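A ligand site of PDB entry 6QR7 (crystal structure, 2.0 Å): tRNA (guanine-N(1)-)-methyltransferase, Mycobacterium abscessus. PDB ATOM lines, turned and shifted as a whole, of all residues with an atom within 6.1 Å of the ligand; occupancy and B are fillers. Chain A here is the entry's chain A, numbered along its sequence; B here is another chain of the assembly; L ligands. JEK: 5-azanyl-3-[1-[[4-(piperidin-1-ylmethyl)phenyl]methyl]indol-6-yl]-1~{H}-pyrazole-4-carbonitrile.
The backbone carbonyl oxygen (O) of Val 133 is in hydrogen-bond range of the backbone NH (N) of Thr 86. The backbone carbonyl oxygen (O) of Gly 136 sits at hydrogen-bond distance from the side-chain hydroxyl (OG) of Ser 134 (3.1 Å). The guanidinium group of Arg 112 is in salt-bridge range of the side-chain carboxylate of Glu 144, at 2.8 Å. The side-chain hydroxyl (OH) of Tyr 138 lies within hydrogen-bond range of the backbone carbonyl oxygen (O) of Ile 135 (3.2 Å). OD1 of Asn 141 sits at hydrogen-bond distance from NE of Arg 156 of chain B (3.1 Å). The backbone NH of Val 133 sits at hydrogen-bond distance from the backbone carbonyl oxygen of Val 84 (3.1 Å). O of Gly 111 is in hydrogen-bond range of N of Gly 143, at 3.0 Å.
The backbone carbonyl oxygen (O) of Gly 136 is in hydrogen-bond range of a nitrogen (N01) of the ligand (2.9 Å). The backbone NH (N) of Ile 135 lies within hydrogen-bond range of a nitrogen (N31) of the ligand, 3.5 Å away. The backbone carbonyl oxygen (O) of Tyr 138 sits at hydrogen-bond distance from a nitrogen (N03) of the ligand, 2.7 Å away. N of Thr 86 lies within hydrogen-bond range of N31 of the ligand (3.4 Å). A nitrogen (N21) of the ligand lies within salt-bridge range of the side-chain carboxylate of Glu 114 (3.4 Å). The backbone NH (N) of Leu 140 is in hydrogen-bond range of a nitrogen (N04) of the ligand (3.0 Å). N01 of the ligand lies within hydrogen-bond range of OG of Ser 134.
O of Val 133 sits close to N31 of the ligand (3.3 Å). O of Pro 85 touches C10 of the ligand, 3.4 Å away. CD of Pro 87 touches C06 of the ligand, 3.6 Å away. O of Gly 111 touches C12 of the ligand, 3.4 Å away. Arg 112 touches the ligand. Tyr 113 touches the ligand. CG1 of Val 139 touches C28 of the ligand, at 3.6 Å. Asn 141 touches the ligand. Gly 142 touches the ligand (CA to C08, 3.5 Å). N of Gly 143 touches C10 of the ligand, at 3.5 Å. CB of Ala 146 touches N31 of the ligand, at 3.5 Å. Glu 182 of chain B touches the ligand (CG to C26, 3.6 Å). Within 4 Å of the ligand: Pro 85, Thr 86, Pro 87, Gly 111, Arg 112, Tyr 113, Glu 114, Val 133, Ser 134, Ile 135, Gly 136, Tyr 138, Val 139, Leu 140, Asn 141, Gly 142, Gly 143, Ala 146 and Glu 182 of chain B.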
ATOM      1  N   PRO A  59      -9.929  11.305 -25.543  1.00  0.00           N
ATOM      2  CA  PRO A  59      -8.738  11.999 -26.034  1.00  0.00           C
ATOM      3  C   PRO A  59      -8.176  12.935 -24.975  1.00  0.00           C
ATOM      4  O   PRO A  59      -8.903  13.327 -24.058  1.00  0.00           O
ATOM      5  CB  PRO A  59      -9.272  12.783 -27.232  1.00  0.00           C
ATOM      6  CG  PRO A  59     -10.663  13.111 -26.845  1.00  0.00           C
ATOM      7  CD  PRO A  59     -11.169  11.937 -26.030  1.00  0.00           C
ATOM      8  N   VAL A  84     -11.568  28.901 -10.754  1.00  0.00           N
ATOM      9  CA  VAL A  84     -11.141  27.846 -11.668  1.00  0.00           C
ATOM     10  C   VAL A  84     -11.670  28.136 -13.080  1.00  0.00           C
ATOM     11  O   VAL A  84     -12.827  27.860 -13.372  1.00  0.00           O
ATOM     12  CB  VAL A  84     -11.644  26.461 -11.210  1.00  0.00           C
ATOM     13  CG1 VAL A  84     -10.978  25.343 -12.064  1.00  0.00           C
ATOM     14  CG2 VAL A  84     -11.345  26.245  -9.730  1.00  0.00           C
ATOM     15  N   PRO A  85     -10.828  28.720 -13.947  1.00  0.00           N
ATOM     16  CA  PRO A  85     -11.298  28.924 -15.322  1.00  0.00           C
ATOM     17  C   PRO A  85     -11.624  27.580 -15.934  1.00  0.00           C
ATOM     18  O   PRO A  85     -10.928  26.603 -15.641  1.00  0.00           O
ATOM     19  CB  PRO A  85     -10.119  29.593 -16.018  1.00  0.00           C
ATOM     20  CG  PRO A  85      -9.341  30.255 -14.877  1.00  0.00           C
ATOM     21  CD  PRO A  85      -9.490  29.293 -13.724  1.00  0.00           C
ATOM     22  N   THR A  86     -12.666  27.519 -16.765  1.00  0.00           N
ATOM     23  CA  THR A  86     -13.053  26.267 -17.439  1.00  0.00           C
ATOM     24  C   THR A  86     -14.043  26.568 -18.551  1.00  0.00           C
ATOM     25  O   THR A  86     -14.893  27.453 -18.407  1.00  0.00           O
ATOM     26  CB  THR A  86     -13.667  25.242 -16.454  1.00  0.00           C
ATOM     27  OG1 THR A  86     -14.353  24.206 -17.183  1.00  0.00           O
ATOM     28  CG2 THR A  86     -14.670  25.923 -15.524  1.00  0.00           C
ATOM     29  N   PRO A  87     -13.948  25.822 -19.666  1.00  0.00           N
ATOM     30  CA  PRO A  87     -14.872  26.069 -20.779  1.00  0.00           C
ATOM     31  C   PRO A  87     -16.284  25.642 -20.396  1.00  0.00           C
ATOM     32  O   PRO A  87     -17.234  25.923 -21.114  1.00  0.00           O
ATOM     33  CB  PRO A  87     -14.296  25.202 -21.908  1.00  0.00           C
ATOM     34  CG  PRO A  87     -13.560  24.115 -21.215  1.00  0.00           C
ATOM     35  CD  PRO A  87     -13.023  24.712 -19.936  1.00  0.00           C
ATOM     36  N   CYS A 110      -5.031  27.587 -12.928  1.00  0.00           N
ATOM     37  CA  CYS A 110      -5.052  27.458 -14.388  1.00  0.00           C
ATOM     38  C   CYS A 110      -4.772  26.036 -14.841  1.00  0.00           C
ATOM     39  O   CYS A 110      -3.651  25.538 -14.679  1.00  0.00           O
ATOM     40  CB  CYS A 110      -4.035  28.401 -15.014  1.00  0.00           C
ATOM     41  SG  CYS A 110      -4.282  30.115 -14.559  1.00  0.00           S
ATOM     42  N   GLY A 111      -5.767  25.396 -15.448  1.00  0.00           N
ATOM     43  CA  GLY A 111      -5.574  24.080 -16.020  1.00  0.00           C
ATOM     44  C   GLY A 111      -4.977  24.105 -17.425  1.00  0.00           C
ATOM     45  O   GLY A 111      -4.879  25.162 -18.061  1.00  0.00           O
ATOM     46  N   ARG A 112      -4.567  22.926 -17.874  1.00  0.00           N
ATOM     47  CA  ARG A 112      -4.161  22.699 -19.256  1.00  0.00           C
ATOM     48  C   ARG A 112      -4.708  21.338 -19.701  1.00  0.00           C
ATOM     49  O   ARG A 112      -5.466  20.723 -18.959  1.00  0.00           O
ATOM     50  CB  ARG A 112      -2.639  22.742 -19.396  1.00  0.00           C
ATOM     51  CG  ARG A 112      -2.071  24.163 -19.431  1.00  0.00           C
ATOM     52  CD  ARG A 112      -1.861  24.634 -20.853  1.00  0.00           C
ATOM     53  NE  ARG A 112      -1.995  26.081 -20.961  1.00  0.00           N
ATOM     54  CZ  ARG A 112      -1.840  26.768 -22.090  1.00  0.00           C
ATOM     55  NH1 ARG A 112      -1.528  26.125 -23.215  1.00  0.00           N
ATOM     56  NH2 ARG A 112      -1.977  28.085 -22.088  1.00  0.00           N
ATOM     57  N   TYR A 113      -4.311  20.883 -20.890  1.00  0.00           N
ATOM     58  CA  TYR A 113      -4.860  19.645 -21.443  1.00  0.00           C
ATOM     59  C   TYR A 113      -6.376  19.678 -21.409  1.00  0.00           C
ATOM     60  O   TYR A 113      -7.001  20.688 -21.745  1.00  0.00           O
ATOM     61  CB  TYR A 113      -4.342  18.431 -20.661  1.00  0.00           C
ATOM     62  CG  TYR A 113      -2.835  18.420 -20.470  1.00  0.00           C
ATOM     63  CD1 TYR A 113      -1.997  17.872 -21.430  1.00  0.00           C
ATOM     64  CD2 TYR A 113      -2.265  18.956 -19.323  1.00  0.00           C
ATOM     65  CE1 TYR A 113      -0.622  17.843 -21.248  1.00  0.00           C
ATOM     66  CE2 TYR A 113      -0.888  18.951 -19.147  1.00  0.00           C
ATOM     67  CZ  TYR A 113      -0.076  18.393 -20.114  1.00  0.00           C
ATOM     68  OH  TYR A 113       1.281  18.376 -19.940  1.00  0.00           O
ATOM     69  N   GLU A 114      -6.992  18.583 -20.982  1.00  0.00           N
ATOM     70  CA  GLU A 114      -8.448  18.510 -20.892  1.00  0.00           C
ATOM     71  C   GLU A 114      -9.006  19.068 -19.586  1.00  0.00           C
ATOM     72  O   GLU A 114     -10.205  19.081 -19.391  1.00  0.00           O
ATOM     73  CB  GLU A 114      -8.931  17.070 -21.051  1.00  0.00           C
ATOM     74  CG  GLU A 114      -8.477  16.448 -22.353  1.00  0.00           C
ATOM     75  CD  GLU A 114      -9.019  17.187 -23.546  1.00  0.00           C
ATOM     76  OE1 GLU A 114      -8.235  17.858 -24.262  1.00  0.00           O
ATOM     77  OE2 GLU A 114     -10.258  17.093 -23.769  1.00  0.00           O
ATOM     78  N   GLY A 115      -8.144  19.553 -18.708  1.00  0.00           N
ATOM     79  CA  GLY A 115      -8.609  20.183 -17.479  1.00  0.00           C
ATOM     80  C   GLY A 115      -8.155  19.436 -16.246  1.00  0.00           C
ATOM     81  O   GLY A 115      -7.264  18.602 -16.306  1.00  0.00           O
ATOM     82  N   ILE A 116      -8.777  19.743 -15.116  1.00  0.00           N
ATOM     83  CA  ILE A 116      -8.368  19.223 -13.830  1.00  0.00           C
ATOM     84  C   ILE A 116      -9.363  18.194 -13.321  1.00  0.00           C
ATOM     85  O   ILE A 116     -10.580  18.412 -13.404  1.00  0.00           O
ATOM     86  CB  ILE A 116      -8.222  20.363 -12.787  1.00  0.00           C
ATOM     87  CG1 ILE A 116      -7.407  21.516 -13.387  1.00  0.00           C
ATOM     88  CG2 ILE A 116      -7.572  19.851 -11.501  1.00  0.00           C
ATOM     89  CD1 ILE A 116      -7.226  22.700 -12.434  1.00  0.00           C
ATOM     90  N   VAL A 133     -15.632  29.193 -13.702  1.00  0.00           N
ATOM     91  CA  VAL A 133     -16.141  30.260 -14.541  1.00  0.00           C
ATOM     92  C   VAL A 133     -15.531  30.187 -15.927  1.00  0.00           C
ATOM     93  O   VAL A 133     -14.414  29.707 -16.091  1.00  0.00           O
ATOM     94  CB  VAL A 133     -15.849  31.675 -13.952  1.00  0.00           C
ATOM     95  CG1 VAL A 133     -16.533  31.847 -12.598  1.00  0.00           C
ATOM     96  CG2 VAL A 133     -14.347  31.919 -13.839  1.00  0.00           C
ATOM     97  N   SER A 134     -16.294  30.660 -16.911  1.00  0.00           N
ATOM     98  CA  SER A 134     -15.786  30.799 -18.268  1.00  0.00           C
ATOM     99  C   SER A 134     -15.827  32.262 -18.712  1.00  0.00           C
ATOM    100  O   SER A 134     -16.829  32.944 -18.473  1.00  0.00           O
ATOM    101  CB  SER A 134     -16.623  29.972 -19.229  1.00  0.00           C
ATOM    102  OG  SER A 134     -16.388  30.394 -20.548  1.00  0.00           O
ATOM    103  N   ILE A 135     -14.784  32.713 -19.395  1.00  0.00           N
ATOM    104  CA  ILE A 135     -14.758  34.113 -19.830  1.00  0.00           C
ATOM    105  C   ILE A 135     -15.447  34.371 -21.169  1.00  0.00           C
ATOM    106  O   ILE A 135     -15.551  35.525 -21.578  1.00  0.00           O
ATOM    107  CB  ILE A 135     -13.320  34.674 -19.930  1.00  0.00           C
ATOM    108  CG1 ILE A 135     -12.492  33.876 -20.943  1.00  0.00           C
ATOM    109  CG2 ILE A 135     -12.667  34.780 -18.548  1.00  0.00           C
ATOM    110  CD1 ILE A 135     -11.332  34.667 -21.568  1.00  0.00           C
ATOM    111  N   GLY A 136     -15.924  33.337 -21.839  1.00  0.00           N
ATOM    112  CA  GLY A 136     -16.649  33.550 -23.089  1.00  0.00           C
ATOM    113  C   GLY A 136     -16.918  32.266 -23.850  1.00  0.00           C
ATOM    114  O   GLY A 136     -16.405  31.205 -23.499  1.00  0.00           O
ATOM    115  N   ASP A 137     -17.705  32.366 -24.924  1.00  0.00           N
ATOM    116  CA  ASP A 137     -18.149  31.191 -25.657  1.00  0.00           C
ATOM    117  C   ASP A 137     -17.222  30.847 -26.810  1.00  0.00           C
ATOM    118  O   ASP A 137     -17.624  30.875 -27.973  1.00  0.00           O
ATOM    119  CB  ASP A 137     -19.589  31.401 -26.140  1.00  0.00           C
ATOM    120  CG  ASP A 137     -20.582  31.388 -24.983  1.00  0.00           C
ATOM    121  OD1 ASP A 137     -20.185  30.956 -23.883  1.00  0.00           O
ATOM    122  OD2 ASP A 137     -21.731  31.807 -25.167  1.00  0.00           O
ATOM    123  N   TYR A 138     -15.987  30.539 -26.461  1.00  0.00           N
ATOM    124  CA  TYR A 138     -14.964  30.099 -27.411  1.00  0.00           C
ATOM    125  C   TYR A 138     -14.059  29.146 -26.638  1.00  0.00           C
ATOM    126  O   TYR A 138     -14.178  29.064 -25.408  1.00  0.00           O
ATOM    127  CB  TYR A 138     -14.165  31.279 -27.971  1.00  0.00           C
ATOM    128  CG  TYR A 138     -13.937  32.351 -26.934  1.00  0.00           C
ATOM    129  CD1 TYR A 138     -12.945  32.225 -25.957  1.00  0.00           C
ATOM    130  CD2 TYR A 138     -14.748  33.468 -26.908  1.00  0.00           C
ATOM    131  CE1 TYR A 138     -12.767  33.223 -24.977  1.00  0.00           C
ATOM    132  CE2 TYR A 138     -14.581  34.463 -25.961  1.00  0.00           C
ATOM    133  CZ  TYR A 138     -13.592  34.334 -24.997  1.00  0.00           C
ATOM    134  OH  TYR A 138     -13.473  35.348 -24.068  1.00  0.00           O
ATOM    135  N   VAL A 139     -13.191  28.431 -27.331  1.00  0.00           N
ATOM    136  CA  VAL A 139     -12.350  27.432 -26.677  1.00  0.00           C
ATOM    137  C   VAL A 139     -10.883  27.848 -26.677  1.00  0.00           C
ATOM    138  O   VAL A 139     -10.335  28.187 -27.724  1.00  0.00           O
ATOM    139  CB  VAL A 139     -12.470  26.040 -27.337  1.00  0.00           C
ATOM    140  CG1 VAL A 139     -11.608  25.032 -26.589  1.00  0.00           C
ATOM    141  CG2 VAL A 139     -13.921  25.552 -27.353  1.00  0.00           C
ATOM    142  N   LEU A 140     -10.257  27.829 -25.511  1.00  0.00           N
ATOM    143  CA  LEU A 140      -8.834  28.167 -25.383  1.00  0.00           C
ATOM    144  C   LEU A 140      -8.004  26.904 -25.153  1.00  0.00           C
ATOM    145  O   LEU A 140      -8.558  25.795 -25.101  1.00  0.00           O
ATOM    146  CB  LEU A 140      -8.640  29.174 -24.238  1.00  0.00           C
ATOM    147  CG  LEU A 140      -9.477  30.463 -24.377  1.00  0.00           C
ATOM    148  CD1 LEU A 140      -9.497  31.246 -23.071  1.00  0.00           C
ATOM    149  CD2 LEU A 140      -8.968  31.345 -25.510  1.00  0.00           C
ATOM    150  N   ASN A 141      -6.699  27.058 -24.985  1.00  0.00           N
ATOM    151  CA  ASN A 141      -5.816  25.930 -24.706  1.00  0.00           C
ATOM    152  C   ASN A 141      -5.646  25.631 -23.221  1.00  0.00           C
ATOM    153  O   ASN A 141      -5.178  24.559 -22.814  1.00  0.00           O
ATOM    154  CB  ASN A 141      -4.442  26.184 -25.315  1.00  0.00           C
ATOM    155  CG  ASN A 141      -4.405  25.935 -26.795  1.00  0.00           C
ATOM    156  OD1 ASN A 141      -5.082  25.036 -27.313  1.00  0.00           O
ATOM    157  ND2 ASN A 141      -3.611  26.721 -27.501  1.00  0.00           N
ATOM    158  N   GLY A 142      -6.010  26.607 -22.389  1.00  0.00           N
ATOM    159  CA  GLY A 142      -5.854  26.461 -20.957  1.00  0.00           C
ATOM    160  C   GLY A 142      -6.356  27.683 -20.222  1.00  0.00           C
ATOM    161  O   GLY A 142      -6.881  28.603 -20.842  1.00  0.00           O
ATOM    162  N   GLY A 143      -6.185  27.705 -18.912  1.00  0.00           N
ATOM    163  CA  GLY A 143      -6.752  28.754 -18.067  1.00  0.00           C
ATOM    164  C   GLY A 143      -5.991  30.066 -18.017  1.00  0.00           C
ATOM    165  O   GLY A 143      -6.516  31.043 -17.495  1.00  0.00           O
ATOM    166  N   GLU A 144      -4.773  30.111 -18.559  1.00  0.00           N
ATOM    167  CA  GLU A 144      -3.887  31.264 -18.349  1.00  0.00           C
ATOM    168  C   GLU A 144      -4.407  32.566 -19.003  1.00  0.00           C
ATOM    169  O   GLU A 144      -4.359  33.639 -18.391  1.00  0.00           O
ATOM    170  CB  GLU A 144      -2.472  30.943 -18.844  1.00  0.00           C
ATOM    171  CG  GLU A 144      -1.673  29.947 -17.984  1.00  0.00           C
ATOM    172  CD  GLU A 144      -2.011  28.473 -18.286  1.00  0.00           C
ATOM    173  OE1 GLU A 144      -2.694  28.204 -19.311  1.00  0.00           O
ATOM    174  OE2 GLU A 144      -1.594  27.577 -17.506  1.00  0.00           O
ATOM    175  N   ALA A 146      -7.479  33.199 -19.614  1.00  0.00           N
ATOM    176  CA  ALA A 146      -8.653  33.561 -18.840  1.00  0.00           C
ATOM    177  C   ALA A 146      -8.247  34.243 -17.542  1.00  0.00           C
ATOM    178  O   ALA A 146      -8.938  35.136 -17.068  1.00  0.00           O
ATOM    179  CB  ALA A 146      -9.505  32.327 -18.546  1.00  0.00           C
ATOM    180  N   ILE A 150      -9.534  37.879 -16.258  1.00  0.00           N
ATOM    181  CA  ILE A 150     -10.167  37.945 -14.940  1.00  0.00           C
ATOM    182  C   ILE A 150      -9.453  38.924 -14.013  1.00  0.00           C
ATOM    183  O   ILE A 150     -10.098  39.761 -13.372  1.00  0.00           O
ATOM    184  CB  ILE A 150     -10.205  36.530 -14.279  1.00  0.00           C
ATOM    185  CG1 ILE A 150     -11.240  35.669 -14.999  1.00  0.00           C
ATOM    186  CG2 ILE A 150     -10.486  36.641 -12.762  1.00  0.00           C
ATOM    187  CD1 ILE A 150     -11.120  34.170 -14.737  1.00  0.00           C
ATOM    188  N   ARG B 156      -5.377  27.842 -32.570  1.00  0.00           N
ATOM    189  CA  ARG B 156      -5.549  26.407 -32.330  1.00  0.00           C
ATOM    190  C   ARG B 156      -6.493  25.751 -33.347  1.00  0.00           C
ATOM    191  O   ARG B 156      -6.635  24.537 -33.382  1.00  0.00           O
ATOM    192  CB  ARG B 156      -6.036  26.156 -30.908  1.00  0.00           C
ATOM    193  CG  ARG B 156      -7.427  26.655 -30.597  1.00  0.00           C
ATOM    194  CD  ARG B 156      -7.761  26.506 -29.107  1.00  0.00           C
ATOM    195  NE  ARG B 156      -7.882  25.123 -28.689  1.00  0.00           N
ATOM    196  CZ  ARG B 156      -8.935  24.353 -28.940  1.00  0.00           C
ATOM    197  NH1 ARG B 156      -9.973  24.831 -29.635  1.00  0.00           N
ATOM    198  NH2 ARG B 156      -8.960  23.092 -28.522  1.00  0.00           N
ATOM    199  N   GLU B 182     -18.958  20.721 -21.441  1.00  0.00           N
ATOM    200  CA  GLU B 182     -18.303  19.464 -21.063  1.00  0.00           C
ATOM    201  C   GLU B 182     -18.583  19.042 -19.625  1.00  0.00           C
ATOM    202  O   GLU B 182     -18.628  19.873 -18.715  1.00  0.00           O
ATOM    203  CB  GLU B 182     -16.786  19.590 -21.279  1.00  0.00           C
ATOM    204  CG  GLU B 182     -16.295  18.890 -22.534  1.00  0.00           C
ATOM    205  CD  GLU B 182     -16.499  17.392 -22.465  1.00  0.00           C
ATOM    206  OE1 GLU B 182     -16.082  16.767 -21.451  1.00  0.00           O
ATOM    207  OE2 GLU B 182     -17.097  16.820 -23.407  1.00  0.00           O
HETATM  208  C10 JEK L   1      -9.399  26.347 -18.708  1.00  0.00           C
HETATM  209  C13 JEK L   1      -7.749  23.375 -20.219  1.00  0.00           C
HETATM  210  C15 JEK L   1      -8.431  23.506 -22.620  1.00  0.00           C
HETATM  211  C17 JEK L   1     -10.233  21.790 -22.072  1.00  0.00           C
HETATM  212  C20 JEK L   1     -13.089  20.249 -24.288  1.00  0.00           C
HETATM  213  C22 JEK L   1     -12.401  19.217 -26.172  1.00  0.00           C
HETATM  214  C24 JEK L   1     -13.133  16.893 -26.281  1.00  0.00           C
HETATM  215  C26 JEK L   1     -13.197  18.052 -24.109  1.00  0.00           C
HETATM  216  C28 JEK L   1     -10.143  22.759 -24.282  1.00  0.00           C
HETATM  217  N01 JEK L   1     -13.832  30.558 -22.222  1.00  0.00           N
HETATM  218  C02 JEK L   1     -12.938  29.523 -22.208  1.00  0.00           C
HETATM  219  N03 JEK L   1     -12.592  28.730 -23.269  1.00  0.00           N
HETATM  220  N04 JEK L   1     -11.673  27.841 -22.837  1.00  0.00           N
HETATM  221  C05 JEK L   1     -11.379  28.063 -21.549  1.00  0.00           C
HETATM  222  C06 JEK L   1     -10.434  27.137 -20.759  1.00  0.00           C
HETATM  223  C07 JEK L   1      -9.897  26.051 -21.443  1.00  0.00           C
HETATM  224  C08 JEK L   1      -9.074  25.119 -20.756  1.00  0.00           C
HETATM  225  C09 JEK L   1      -8.835  25.261 -19.404  1.00  0.00           C
HETATM  226  C11 JEK L   1     -10.215  27.276 -19.388  1.00  0.00           C
HETATM  227  C12 JEK L   1      -7.969  24.134 -19.048  1.00  0.00           C
HETATM  228  N14 JEK L   1      -8.411  23.963 -21.211  1.00  0.00           N
HETATM  229  C16 JEK L   1      -9.648  22.655 -22.979  1.00  0.00           C
HETATM  230  C18 JEK L   1     -11.341  21.007 -22.480  1.00  0.00           C
HETATM  231  C19 JEK L   1     -11.852  21.114 -23.811  1.00  0.00           C
HETATM  232  N21 JEK L   1     -12.679  19.218 -24.733  1.00  0.00           N
HETATM  233  C23 JEK L   1     -13.075  18.116 -26.983  1.00  0.00           C
HETATM  234  C25 JEK L   1     -13.883  17.062 -25.039  1.00  0.00           C
HETATM  235  C27 JEK L   1     -11.263  21.961 -24.685  1.00  0.00           C
HETATM  236  C29 JEK L   1     -12.183  29.085 -21.112  1.00  0.00           C
HETATM  237  C30 JEK L   1     -12.281  29.770 -19.696  1.00  0.00           C
HETATM  238  N31 JEK L   1     -12.393  30.299 -18.669  1.00  0.00           N
